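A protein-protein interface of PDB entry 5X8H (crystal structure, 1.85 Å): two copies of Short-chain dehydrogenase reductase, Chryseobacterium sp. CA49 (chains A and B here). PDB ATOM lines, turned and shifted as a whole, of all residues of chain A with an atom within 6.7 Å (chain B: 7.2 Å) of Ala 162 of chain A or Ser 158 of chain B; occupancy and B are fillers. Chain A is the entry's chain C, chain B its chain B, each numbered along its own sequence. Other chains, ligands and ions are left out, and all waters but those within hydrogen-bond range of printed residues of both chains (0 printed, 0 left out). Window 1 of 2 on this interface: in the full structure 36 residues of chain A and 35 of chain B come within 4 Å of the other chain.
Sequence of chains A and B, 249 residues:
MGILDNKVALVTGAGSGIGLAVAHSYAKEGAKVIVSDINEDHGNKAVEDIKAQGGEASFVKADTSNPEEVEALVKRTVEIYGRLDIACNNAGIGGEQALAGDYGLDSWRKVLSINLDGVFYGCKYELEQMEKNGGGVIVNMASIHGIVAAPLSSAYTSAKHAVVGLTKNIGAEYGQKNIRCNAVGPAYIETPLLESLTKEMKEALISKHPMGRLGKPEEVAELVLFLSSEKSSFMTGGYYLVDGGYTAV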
ATOM      1  N   LEU A 112      -3.114   8.218 -23.618  1.00  0.00           N
ATOM      2  CA  LEU A 112      -3.218   6.755 -23.532  1.00  0.00           C
ATOM      3  C   LEU A 112      -2.207   6.018 -24.368  1.00  0.00           C
ATOM      4  O   LEU A 112      -1.702   4.937 -23.977  1.00  0.00           O
ATOM      5  CB  LEU A 112      -4.619   6.261 -23.910  1.00  0.00           C
ATOM      6  CG  LEU A 112      -5.645   6.182 -22.788  1.00  0.00           C
ATOM      7  CD1 LEU A 112      -5.229   5.093 -21.808  1.00  0.00           C
ATOM      8  CD2 LEU A 112      -5.843   7.514 -22.078  1.00  0.00           C
ATOM      9  N   LEU A 116      -0.104   4.344 -21.564  1.00  0.00           N
ATOM     10  CA  LEU A 116      -0.490   2.996 -21.413  1.00  0.00           C
ATOM     11  C   LEU A 116       0.086   2.153 -22.532  1.00  0.00           C
ATOM     12  O   LEU A 116       0.853   1.251 -22.256  1.00  0.00           O
ATOM     13  CB  LEU A 116      -1.996   2.847 -21.293  1.00  0.00           C
ATOM     14  CG  LEU A 116      -2.527   1.411 -21.369  1.00  0.00           C
ATOM     15  CD1 LEU A 116      -1.987   0.591 -20.216  1.00  0.00           C
ATOM     16  CD2 LEU A 116      -4.022   1.329 -21.474  1.00  0.00           C
ATOM     17  N   PHE A 120       2.623  -1.088 -22.316  1.00  0.00           N
ATOM     18  CA  PHE A 120       2.313  -2.446 -22.779  1.00  0.00           C
ATOM     19  C   PHE A 120       3.333  -2.920 -23.838  1.00  0.00           C
ATOM     20  O   PHE A 120       3.858  -4.038 -23.741  1.00  0.00           O
ATOM     21  CB  PHE A 120       0.876  -2.550 -23.292  1.00  0.00           C
ATOM     22  CG  PHE A 120       0.629  -3.723 -24.190  1.00  0.00           C
ATOM     23  CD1 PHE A 120       0.702  -5.006 -23.709  1.00  0.00           C
ATOM     24  CD2 PHE A 120       0.336  -3.526 -25.543  1.00  0.00           C
ATOM     25  CE1 PHE A 120       0.484  -6.097 -24.545  1.00  0.00           C
ATOM     26  CE2 PHE A 120       0.133  -4.612 -26.396  1.00  0.00           C
ATOM     27  CZ  PHE A 120       0.205  -5.901 -25.891  1.00  0.00           C
ATOM     28  N   GLY A 146      -2.590   6.380 -10.466  1.00  0.00           N
ATOM     29  CA  GLY A 146      -3.031   5.014 -10.710  1.00  0.00           C
ATOM     30  C   GLY A 146      -4.008   4.540  -9.664  1.00  0.00           C
ATOM     31  O   GLY A 146      -4.583   3.462  -9.835  1.00  0.00           O
ATOM     32  N   THR A 157      -5.004   9.854 -15.446  1.00  0.00           N
ATOM     33  CA  THR A 157      -5.476   9.005 -14.397  1.00  0.00           C
ATOM     34  C   THR A 157      -5.901   7.635 -14.925  1.00  0.00           C
ATOM     35  O   THR A 157      -5.529   6.569 -14.384  1.00  0.00           O
ATOM     36  CB  THR A 157      -6.650   9.686 -13.747  1.00  0.00           C
ATOM     37  OG1 THR A 157      -6.184  10.942 -13.204  1.00  0.00           O
ATOM     38  CG2 THR A 157      -7.294   8.764 -12.695  1.00  0.00           C
ATOM     39  N   SER A 158      -6.659   7.666 -16.005  1.00  0.00           N
ATOM     40  CA  SER A 158      -7.111   6.434 -16.644  1.00  0.00           C
ATOM     41  C   SER A 158      -5.934   5.602 -17.101  1.00  0.00           C
ATOM     42  O   SER A 158      -5.889   4.345 -16.898  1.00  0.00           O
ATOM     43  CB  SER A 158      -8.020   6.770 -17.815  1.00  0.00           C
ATOM     44  OG  SER A 158      -9.148   7.463 -17.418  1.00  0.00           O
ATOM     45  N   ALA A 159      -4.935   6.237 -17.716  1.00  0.00           N
ATOM     46  CA  ALA A 159      -3.831   5.482 -18.271  1.00  0.00           C
ATOM     47  C   ALA A 159      -3.003   4.895 -17.120  1.00  0.00           C
ATOM     48  O   ALA A 159      -2.574   3.766 -17.169  1.00  0.00           O
ATOM     49  CB  ALA A 159      -2.936   6.374 -19.157  1.00  0.00           C
ATOM     50  N   LYS A 160      -2.776   5.673 -16.065  1.00  0.00           N
ATOM     51  CA  LYS A 160      -1.942   5.152 -14.946  1.00  0.00           C
ATOM     52  C   LYS A 160      -2.667   4.029 -14.172  1.00  0.00           C
ATOM     53  O   LYS A 160      -2.057   3.063 -13.704  1.00  0.00           O
ATOM     54  CB  LYS A 160      -1.537   6.300 -14.013  1.00  0.00           C
ATOM     55  CG  LYS A 160      -0.611   7.348 -14.611  1.00  0.00           C
ATOM     56  CD  LYS A 160       0.622   6.771 -15.193  1.00  0.00           C
ATOM     57  CE  LYS A 160       1.654   7.823 -15.573  1.00  0.00           C
ATOM     58  NZ  LYS A 160       2.945   7.157 -15.848  1.00  0.00           N
ATOM     59  N   HIS A 161      -3.979   4.142 -14.060  1.00  0.00           N
ATOM     60  CA  HIS A 161      -4.794   3.043 -13.507  1.00  0.00           C
ATOM     61  C   HIS A 161      -4.606   1.750 -14.316  1.00  0.00           C
ATOM     62  O   HIS A 161      -4.373   0.692 -13.733  1.00  0.00           O
ATOM     63  CB  HIS A 161      -6.257   3.445 -13.483  1.00  0.00           C
ATOM     64  CG  HIS A 161      -6.692   4.087 -12.188  1.00  0.00           C
ATOM     65  ND1 HIS A 161      -6.355   5.373 -11.832  1.00  0.00           N
ATOM     66  CD2 HIS A 161      -7.555   3.658 -11.247  1.00  0.00           C
ATOM     67  CE1 HIS A 161      -6.911   5.674 -10.675  1.00  0.00           C
ATOM     68  NE2 HIS A 161      -7.652   4.647 -10.308  1.00  0.00           N
ATOM     69  N   ALA A 162      -4.669   1.875 -15.642  1.00  0.00           N
ATOM     70  CA  ALA A 162      -4.431   0.723 -16.554  1.00  0.00           C
ATOM     71  C   ALA A 162      -3.038   0.111 -16.343  1.00  0.00           C
ATOM     72  O   ALA A 162      -2.856  -1.095 -16.422  1.00  0.00           O
ATOM     73  CB  ALA A 162      -4.587   1.164 -17.996  1.00  0.00           C
ATOM     74  N   VAL A 163      -2.037   0.955 -16.137  1.00  0.00           N
ATOM     75  CA  VAL A 163      -0.685   0.477 -15.845  1.00  0.00           C
ATOM     76  C   VAL A 163      -0.660  -0.406 -14.636  1.00  0.00           C
ATOM     77  O   VAL A 163       0.018  -1.434 -14.635  1.00  0.00           O
ATOM     78  CB  VAL A 163       0.338   1.645 -15.674  1.00  0.00           C
ATOM     79  CG1 VAL A 163       1.657   1.131 -15.146  1.00  0.00           C
ATOM     80  CG2 VAL A 163       0.537   2.335 -17.022  1.00  0.00           C
ATOM     81  N   VAL A 164      -1.368   0.019 -13.591  1.00  0.00           N
ATOM     82  CA  VAL A 164      -1.474  -0.739 -12.382  1.00  0.00           C
ATOM     83  C   VAL A 164      -2.109  -2.100 -12.615  1.00  0.00           C
ATOM     84  O   VAL A 164      -1.609  -3.091 -12.101  1.00  0.00           O
ATOM     85  CB  VAL A 164      -2.279   0.039 -11.277  1.00  0.00           C
ATOM     86  CG1 VAL A 164      -2.509  -0.832 -10.052  1.00  0.00           C
ATOM     87  CG2 VAL A 164      -1.529   1.320 -10.895  1.00  0.00           C
ATOM     88  N   GLY A 165      -3.189  -2.138 -13.375  1.00  0.00           N
ATOM     89  CA  GLY A 165      -3.816  -3.404 -13.795  1.00  0.00           C
ATOM     90  C   GLY A 165      -2.928  -4.280 -14.660  1.00  0.00           C
ATOM     91  O   GLY A 165      -2.813  -5.458 -14.395  1.00  0.00           O
ATOM     92  N   LEU A 166      -2.208  -3.667 -15.601  1.00  0.00           N
ATOM     93  CA  LEU A 166      -1.288  -4.388 -16.467  1.00  0.00           C
ATOM     94  C   LEU A 166      -0.237  -5.066 -15.615  1.00  0.00           C
ATOM     95  O   LEU A 166       0.131  -6.217 -15.849  1.00  0.00           O
ATOM     96  CB  LEU A 166      -0.643  -3.450 -17.427  1.00  0.00           C
ATOM     97  CG  LEU A 166       0.380  -4.021 -18.404  1.00  0.00           C
ATOM     98  CD1 LEU A 166      -0.211  -5.165 -19.236  1.00  0.00           C
ATOM     99  CD2 LEU A 166       0.963  -2.936 -19.289  1.00  0.00           C
ATOM    100  N   THR A 167       0.274  -4.314 -14.634  1.00  0.00           N
ATOM    101  CA  THR A 167       1.308  -4.822 -13.711  1.00  0.00           C
ATOM    102  C   THR A 167       0.843  -6.025 -12.932  1.00  0.00           C
ATOM    103  O   THR A 167       1.607  -7.000 -12.786  1.00  0.00           O
ATOM    104  CB  THR A 167       1.771  -3.662 -12.804  1.00  0.00           C
ATOM    105  OG1 THR A 167       2.336  -2.638 -13.651  1.00  0.00           O
ATOM    106  CG2 THR A 167       2.801  -4.069 -11.764  1.00  0.00           C
ATOM    107  N   ASN A 169      -1.509  -8.112 -13.757  1.00  0.00           N
ATOM    108  CA  ASN A 169      -1.576  -9.193 -14.750  1.00  0.00           C
ATOM    109  C   ASN A 169      -0.263  -9.867 -15.087  1.00  0.00           C
ATOM    110  O   ASN A 169      -0.172 -11.093 -15.096  1.00  0.00           O
ATOM    111  CB  ASN A 169      -2.259  -8.726 -16.048  1.00  0.00           C
ATOM    112  CG  ASN A 169      -3.611  -9.350 -16.225  1.00  0.00           C
ATOM    113  OD1 ASN A 169      -4.584  -8.987 -15.551  1.00  0.00           O
ATOM    114  ND2 ASN A 169      -3.692 -10.326 -17.129  1.00  0.00           N
ATOM    115  N   TRP B 108      -4.949  -6.006 -28.415  1.00  0.00           N
ATOM    116  CA  TRP B 108      -4.757  -4.992 -27.359  1.00  0.00           C
ATOM    117  C   TRP B 108      -5.518  -3.741 -27.713  1.00  0.00           C
ATOM    118  O   TRP B 108      -6.421  -3.302 -26.977  1.00  0.00           O
ATOM    119  CB  TRP B 108      -3.267  -4.665 -27.141  1.00  0.00           C
ATOM    120  CG  TRP B 108      -3.066  -3.576 -26.110  1.00  0.00           C
ATOM    121  CD1 TRP B 108      -3.052  -2.223 -26.346  1.00  0.00           C
ATOM    122  CD2 TRP B 108      -2.895  -3.733 -24.671  1.00  0.00           C
ATOM    123  NE1 TRP B 108      -2.892  -1.555 -25.174  1.00  0.00           N
ATOM    124  CE2 TRP B 108      -2.778  -2.448 -24.135  1.00  0.00           C
ATOM    125  CE3 TRP B 108      -2.806  -4.839 -23.809  1.00  0.00           C
ATOM    126  CZ2 TRP B 108      -2.616  -2.213 -22.749  1.00  0.00           C
ATOM    127  CZ3 TRP B 108      -2.621  -4.621 -22.409  1.00  0.00           C
ATOM    128  CH2 TRP B 108      -2.527  -3.308 -21.909  1.00  0.00           C
ATOM    129  N   VAL B 111      -9.400  -4.146 -27.681  1.00  0.00           N
ATOM    130  CA  VAL B 111      -9.965  -4.200 -26.330  1.00  0.00           C
ATOM    131  C   VAL B 111      -9.962  -2.809 -25.688  1.00  0.00           C
ATOM    132  O   VAL B 111     -10.962  -2.407 -25.125  1.00  0.00           O
ATOM    133  CB  VAL B 111      -9.268  -5.259 -25.468  1.00  0.00           C
ATOM    134  CG1 VAL B 111      -9.711  -5.169 -24.021  1.00  0.00           C
ATOM    135  CG2 VAL B 111      -9.611  -6.660 -25.998  1.00  0.00           C
ATOM    136  N   LEU B 112      -8.841  -2.101 -25.752  1.00  0.00           N
ATOM    137  CA  LEU B 112      -8.750  -0.767 -25.130  1.00  0.00           C
ATOM    138  C   LEU B 112      -9.676   0.221 -25.830  1.00  0.00           C
ATOM    139  O   LEU B 112     -10.339   1.041 -25.184  1.00  0.00           O
ATOM    140  CB  LEU B 112      -7.329  -0.232 -25.135  1.00  0.00           C
ATOM    141  CG  LEU B 112      -6.470  -0.573 -23.921  1.00  0.00           C
ATOM    142  CD1 LEU B 112      -6.965   0.133 -22.654  1.00  0.00           C
ATOM    143  CD2 LEU B 112      -6.430  -2.076 -23.699  1.00  0.00           C
ATOM    144  N   LEU B 116     -12.292   0.892 -22.906  1.00  0.00           N
ATOM    145  CA  LEU B 116     -11.904   2.184 -22.334  1.00  0.00           C
ATOM    146  C   LEU B 116     -12.335   3.356 -23.216  1.00  0.00           C
ATOM    147  O   LEU B 116     -13.127   4.163 -22.787  1.00  0.00           O
ATOM    148  CB  LEU B 116     -10.404   2.270 -22.037  1.00  0.00           C
ATOM    149  CG  LEU B 116      -9.923   3.630 -21.530  1.00  0.00           C
ATOM    150  CD1 LEU B 116     -10.696   4.031 -20.270  1.00  0.00           C
ATOM    151  CD2 LEU B 116      -8.430   3.656 -21.311  1.00  0.00           C
ATOM    152  N   HIS B 145     -12.075  -7.176 -12.461  1.00  0.00           N
ATOM    153  CA  HIS B 145     -10.801  -6.937 -13.106  1.00  0.00           C
ATOM    154  C   HIS B 145     -10.404  -5.497 -13.355  1.00  0.00           C
ATOM    155  O   HIS B 145      -9.370  -5.235 -13.983  1.00  0.00           O
ATOM    156  CB  HIS B 145     -10.685  -7.833 -14.334  1.00  0.00           C
ATOM    157  CG  HIS B 145     -10.856  -9.272 -13.984  1.00  0.00           C
ATOM    158  ND1 HIS B 145     -10.104  -9.864 -12.985  1.00  0.00           N
ATOM    159  CD2 HIS B 145     -11.772 -10.192 -14.362  1.00  0.00           C
ATOM    160  CE1 HIS B 145     -10.477 -11.119 -12.853  1.00  0.00           C
ATOM    161  NE2 HIS B 145     -11.500 -11.332 -13.647  1.00  0.00           N
ATOM    162  N   GLY B 146     -11.211  -4.596 -12.812  1.00  0.00           N
ATOM    163  CA  GLY B 146     -10.801  -3.246 -12.576  1.00  0.00           C
ATOM    164  C   GLY B 146     -10.008  -3.078 -11.295  1.00  0.00           C
ATOM    165  O   GLY B 146      -9.446  -1.999 -11.082  1.00  0.00           O
ATOM    166  N   SER B 153      -5.775 -12.167 -19.791  1.00  0.00           N
ATOM    167  CA  SER B 153      -6.665 -11.127 -20.281  1.00  0.00           C
ATOM    168  C   SER B 153      -6.101  -9.753 -19.821  1.00  0.00           C
ATOM    169  O   SER B 153      -6.814  -8.960 -19.157  1.00  0.00           O
ATOM    170  CB  SER B 153      -8.073 -11.353 -19.758  1.00  0.00           C
ATOM    171  OG  SER B 153      -8.658 -12.554 -20.247  1.00  0.00           O
ATOM    172  N   SER B 154      -4.853  -9.461 -20.167  1.00  0.00           N
ATOM    173  CA  SER B 154      -4.210  -8.197 -19.689  1.00  0.00           C
ATOM    174  C   SER B 154      -4.884  -6.940 -20.237  1.00  0.00           C
ATOM    175  O   SER B 154      -5.010  -5.935 -19.522  1.00  0.00           O
ATOM    176  CB  SER B 154      -2.749  -8.152 -19.985  1.00  0.00           C
ATOM    177  OG  SER B 154      -2.469  -8.417 -21.307  1.00  0.00           O
ATOM    178  N   ALA B 155      -5.314  -6.992 -21.494  1.00  0.00           N
ATOM    179  CA  ALA B 155      -5.979  -5.860 -22.092  1.00  0.00           C
ATOM    180  C   ALA B 155      -7.276  -5.541 -21.432  1.00  0.00           C
ATOM    181  O   ALA B 155      -7.570  -4.366 -21.173  1.00  0.00           O
ATOM    182  CB  ALA B 155      -6.179  -6.069 -23.573  1.00  0.00           C
ATOM    183  N   TYR B 156      -8.072  -6.575 -21.156  1.00  0.00           N
ATOM    184  CA  TYR B 156      -9.323  -6.409 -20.450  1.00  0.00           C
ATOM    185  C   TYR B 156      -9.099  -5.772 -19.063  1.00  0.00           C
ATOM    186  O   TYR B 156      -9.757  -4.806 -18.678  1.00  0.00           O
ATOM    187  CB  TYR B 156     -10.042  -7.751 -20.334  1.00  0.00           C
ATOM    188  CG  TYR B 156     -11.390  -7.688 -19.706  1.00  0.00           C
ATOM    189  CD1 TYR B 156     -12.535  -7.372 -20.479  1.00  0.00           C
ATOM    190  CD2 TYR B 156     -11.564  -8.000 -18.376  1.00  0.00           C
ATOM    191  CE1 TYR B 156     -13.770  -7.317 -19.916  1.00  0.00           C
ATOM    192  CE2 TYR B 156     -12.824  -7.934 -17.797  1.00  0.00           C
ATOM    193  CZ  TYR B 156     -13.905  -7.561 -18.564  1.00  0.00           C
ATOM    194  OH  TYR B 156     -15.110  -7.508 -17.993  1.00  0.00           O
ATOM    195  N   THR B 157      -8.180  -6.345 -18.322  1.00  0.00           N
ATOM    196  CA  THR B 157      -7.836  -5.850 -16.963  1.00  0.00           C
ATOM    197  C   THR B 157      -7.394  -4.394 -16.978  1.00  0.00           C
ATOM    198  O   THR B 157      -7.795  -3.587 -16.116  1.00  0.00           O
ATOM    199  CB  THR B 157      -6.723  -6.734 -16.361  1.00  0.00           C
ATOM    200  OG1 THR B 157      -7.159  -8.114 -16.316  1.00  0.00           O
ATOM    201  CG2 THR B 157      -6.298  -6.299 -14.963  1.00  0.00           C
ATOM    202  N   SER B 158      -6.532  -4.061 -17.931  1.00  0.00           N
ATOM    203  CA  SER B 158      -5.967  -2.716 -18.053  1.00  0.00           C
ATOM    204  C   SER B 158      -7.056  -1.718 -18.380  1.00  0.00           C
ATOM    205  O   SER B 158      -7.161  -0.661 -17.753  1.00  0.00           O
ATOM    206  CB  SER B 158      -4.868  -2.706 -19.128  1.00  0.00           C
ATOM    207  OG  SER B 158      -3.829  -3.621 -18.813  1.00  0.00           O
ATOM    208  N   ALA B 159      -7.935  -2.101 -19.303  1.00  0.00           N
ATOM    209  CA  ALA B 159      -9.075  -1.245 -19.686  1.00  0.00           C
ATOM    210  C   ALA B 159     -10.042  -1.050 -18.525  1.00  0.00           C
ATOM    211  O   ALA B 159     -10.520   0.052 -18.269  1.00  0.00           O
ATOM    212  CB  ALA B 159      -9.811  -1.861 -20.879  1.00  0.00           C
ATOM    213  N   LYS B 160     -10.359  -2.115 -17.800  1.00  0.00           N
ATOM    214  CA  LYS B 160     -11.317  -1.969 -16.721  1.00  0.00           C
ATOM    215  C   LYS B 160     -10.727  -1.198 -15.518  1.00  0.00           C
ATOM    216  O   LYS B 160     -11.471  -0.467 -14.863  1.00  0.00           O
ATOM    217  CB  LYS B 160     -11.892  -3.293 -16.268  1.00  0.00           C
ATOM    218  CG  LYS B 160     -12.716  -4.036 -17.313  1.00  0.00           C
ATOM    219  CD  LYS B 160     -13.884  -3.233 -17.813  1.00  0.00           C
ATOM    220  CE  LYS B 160     -14.979  -4.092 -18.461  1.00  0.00           C
ATOM    221  NZ  LYS B 160     -16.088  -3.214 -18.906  1.00  0.00           N
ATOM    222  N   HIS B 161      -9.439  -1.380 -15.258  1.00  0.00           N
ATOM    223  CA  HIS B 161      -8.709  -0.508 -14.299  1.00  0.00           C
ATOM    224  C   HIS B 161      -8.855   0.957 -14.724  1.00  0.00           C
ATOM    225  O   HIS B 161      -9.284   1.792 -13.929  1.00  0.00           O
ATOM    226  CB  HIS B 161      -7.273  -0.856 -14.229  1.00  0.00           C
ATOM    227  CG  HIS B 161      -6.959  -1.891 -13.213  1.00  0.00           C
ATOM    228  ND1 HIS B 161      -7.413  -3.188 -13.313  1.00  0.00           N
ATOM    229  CD2 HIS B 161      -6.220  -1.831 -12.074  1.00  0.00           C
ATOM    230  CE1 HIS B 161      -6.995  -3.876 -12.274  1.00  0.00           C
ATOM    231  NE2 HIS B 161      -6.281  -3.063 -11.500  1.00  0.00           N
ATOM    232  N   ALA B 162      -8.559   1.241 -15.989  1.00  0.00           N
ATOM    233  CA  ALA B 162      -8.733   2.591 -16.538  1.00  0.00           C
ATOM    234  C   ALA B 162     -10.144   3.150 -16.355  1.00  0.00           C
ATOM    235  O   ALA B 162     -10.290   4.319 -16.045  1.00  0.00           O
ATOM    236  CB  ALA B 162      -8.310   2.664 -17.993  1.00  0.00           C
ATOM    237  N   VAL B 163     -11.175   2.326 -16.543  1.00  0.00           N
ATOM    238  CA  VAL B 163     -12.553   2.732 -16.299  1.00  0.00           C
ATOM    239  C   VAL B 163     -12.796   3.173 -14.833  1.00  0.00           C
ATOM    240  O   VAL B 163     -13.465   4.155 -14.575  1.00  0.00           O
ATOM    241  CB  VAL B 163     -13.533   1.620 -16.761  1.00  0.00           C
ATOM    242  CG1 VAL B 163     -14.932   1.829 -16.246  1.00  0.00           C
ATOM    243  CG2 VAL B 163     -13.547   1.533 -18.269  1.00  0.00           C
ATOM    244  N   VAL B 164     -12.189   2.480 -13.868  1.00  0.00           N
ATOM    245  CA  VAL B 164     -12.317   2.851 -12.477  1.00  0.00           C
ATOM    246  C   VAL B 164     -11.666   4.227 -12.279  1.00  0.00           C
ATOM    247  O   VAL B 164     -12.243   5.116 -11.647  1.00  0.00           O
ATOM    248  CB  VAL B 164     -11.647   1.783 -11.605  1.00  0.00           C
ATOM    249  CG1 VAL B 164     -11.591   2.255 -10.177  1.00  0.00           C
ATOM    250  CG2 VAL B 164     -12.420   0.426 -11.714  1.00  0.00           C
ATOM    251  N   GLY B 165     -10.494   4.428 -12.885  1.00  0.00           N
ATOM    252  CA  GLY B 165      -9.783   5.714 -12.752  1.00  0.00           C
ATOM    253  C   GLY B 165     -10.558   6.878 -13.372  1.00  0.00           C
ATOM    254  O   GLY B 165     -10.777   7.926 -12.735  1.00  0.00           O
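The side-chain amide nitrogen of Asn 169 of chain A sits close to the backbone NH of Ser 154 of chain B, 3.4 Å away. OG1 of Thr 157 of chain B is in hydrogen-bond range of OD1 of Asn 169 of chain A.
O of His 145 of chain B is in hydrogen-bond range of ND1 of His 161 of chain B, at 2.9 Å. A ring nitrogen (ND1) of His 161 of chain B sits at hydrogen-bond distance from the backbone carbonyl oxygen (O) of Gly 146 of chain B, at 3.2 Å. The backbone carbonyl oxygen (O) of Ser 153 of chain B lies within hydrogen-bond range of the side-chain hydroxyl (OG1) of Thr 157 of chain B (3.0 Å). The backbone carbonyl oxygen (O) of Ser 154 of chain B sits at hydrogen-bond distance from the side-chain hydroxyl (OG) of Ser 158 of chain B (2.7 Å). O of Gly 146 of chain A lies close to ND1 of His 161 of chain A, 3.3 Å away. A ring nitrogen (ND1) of His 161 of chain A lies within hydrogen-bond range of the backbone carbonyl oxygen (O) of Thr 157 of chain A (2.9 Å).
Among the printed residues, pairs that only touch across the chains: Leu 112 of chain A with Leu 116 of chain B (3.5 Å), Leu 116 of chain A with Trp 108 of chain B (3.8 Å), Leu 116 of chain A with Leu 112 of chain B (3.4 Å), Phe 120 of chain A with Trp 108 of chain B (3.4 Å), Thr 157 of chain A with Gly 165 of chain B (3.6 Å), Ser 158 of chain A with Ala 162 of chain B (3.1 Å), His 161 of chain A with His 161 of chain B (3.3 Å), His 161 of chain A with Gly 165 of chain B (3.4 Å), Ala 162 of chain A with Ser 158 of chain B (3.2 Å), Ala 162 of chain A with His 161 of chain B (3.997 Å), Ala 162 of chain A with Ala 162 of chain B (3.96 Å), Gly 165 of chain A with Thr 157 of chain B (3.6 Å), Gly 165 of chain A with His 161 of chain B (3.3 Å), Leu 166 of chain A with Trp 108 of chain B (3.99 Å), Leu 166 of chain A with Ser 154 of chain B (3.99 Å), Leu 166 of chain A with Ser 158 of chain B (3.5 Å) and Asn 169 of chain A with Ser 153 of chain B (3.7 Å).
Printed residues of chain B within 4 Å of Ala 162 of chain A: Ser 158, His 161 and Ala 162. Ser 158 of chain B touches just these residues of chain A: Ala 162 (3.2 Å) and Leu 166 (3.5 Å). Of the printed residues of chain B, Leu 166 of chain A touches Trp 108 (3.99 Å), Ser 154 (3.99 Å) and Ser 158 (3.5 Å). Of the printed residues of chain B, Ser 158 of chain A touches Ala 162. Printed residues of chain A within 4 Å of Thr 157 of chain B: Gly 165 and Asn 169. Ala 159 of chain A touches none of the printed residues of chain B. Val 111 of chain B touches none of the printed residues of chain A. The nearest printed residue of chain B that does not touch His 161 of chain A is Ala 162 of chain B (4.02 Å).
Of the 16 printed residues of chain A, 10 touch a printed residue of chain B. Hydrophobic or aromatic side chains of chain A within 4 Å of the printed part of chain B: Leu 112, Leu 116, Phe 120, His 161, Ala 162 and Leu 166. Of the 19 printed residues of chain B, 10 touch a printed residue of chain A. Along chain B the printed residues that touch a printed residue of chain A span positions 108 to 165. Among the printed residues, no Asp or Glu carboxylate lies within 4 Å of a Lys or Arg side-chain nitrogen of the other chain.
Leu 112 of chain A touches Leu 116 of chain B, and with the chains exchanged Leu 116 of chain A touches Leu 112 of chain B. Thr 157 of chain A touches Gly 165 of chain B, and with the chains exchanged Gly 165 of chain A touches Thr 157 of chain B. Ser 158 of chain A touches Ala 162 of chain B, and with the chains exchanged Ala 162 of chain A touches Ser 158 of chain B. Ala 162 of chain B touches its own counterpart, Ala 162 of chain A. 12 positions are printed for both chains. Of the 19 pairs that touch across the chains among the printed residues, 10 have their exchanged pair printed and touching as well.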
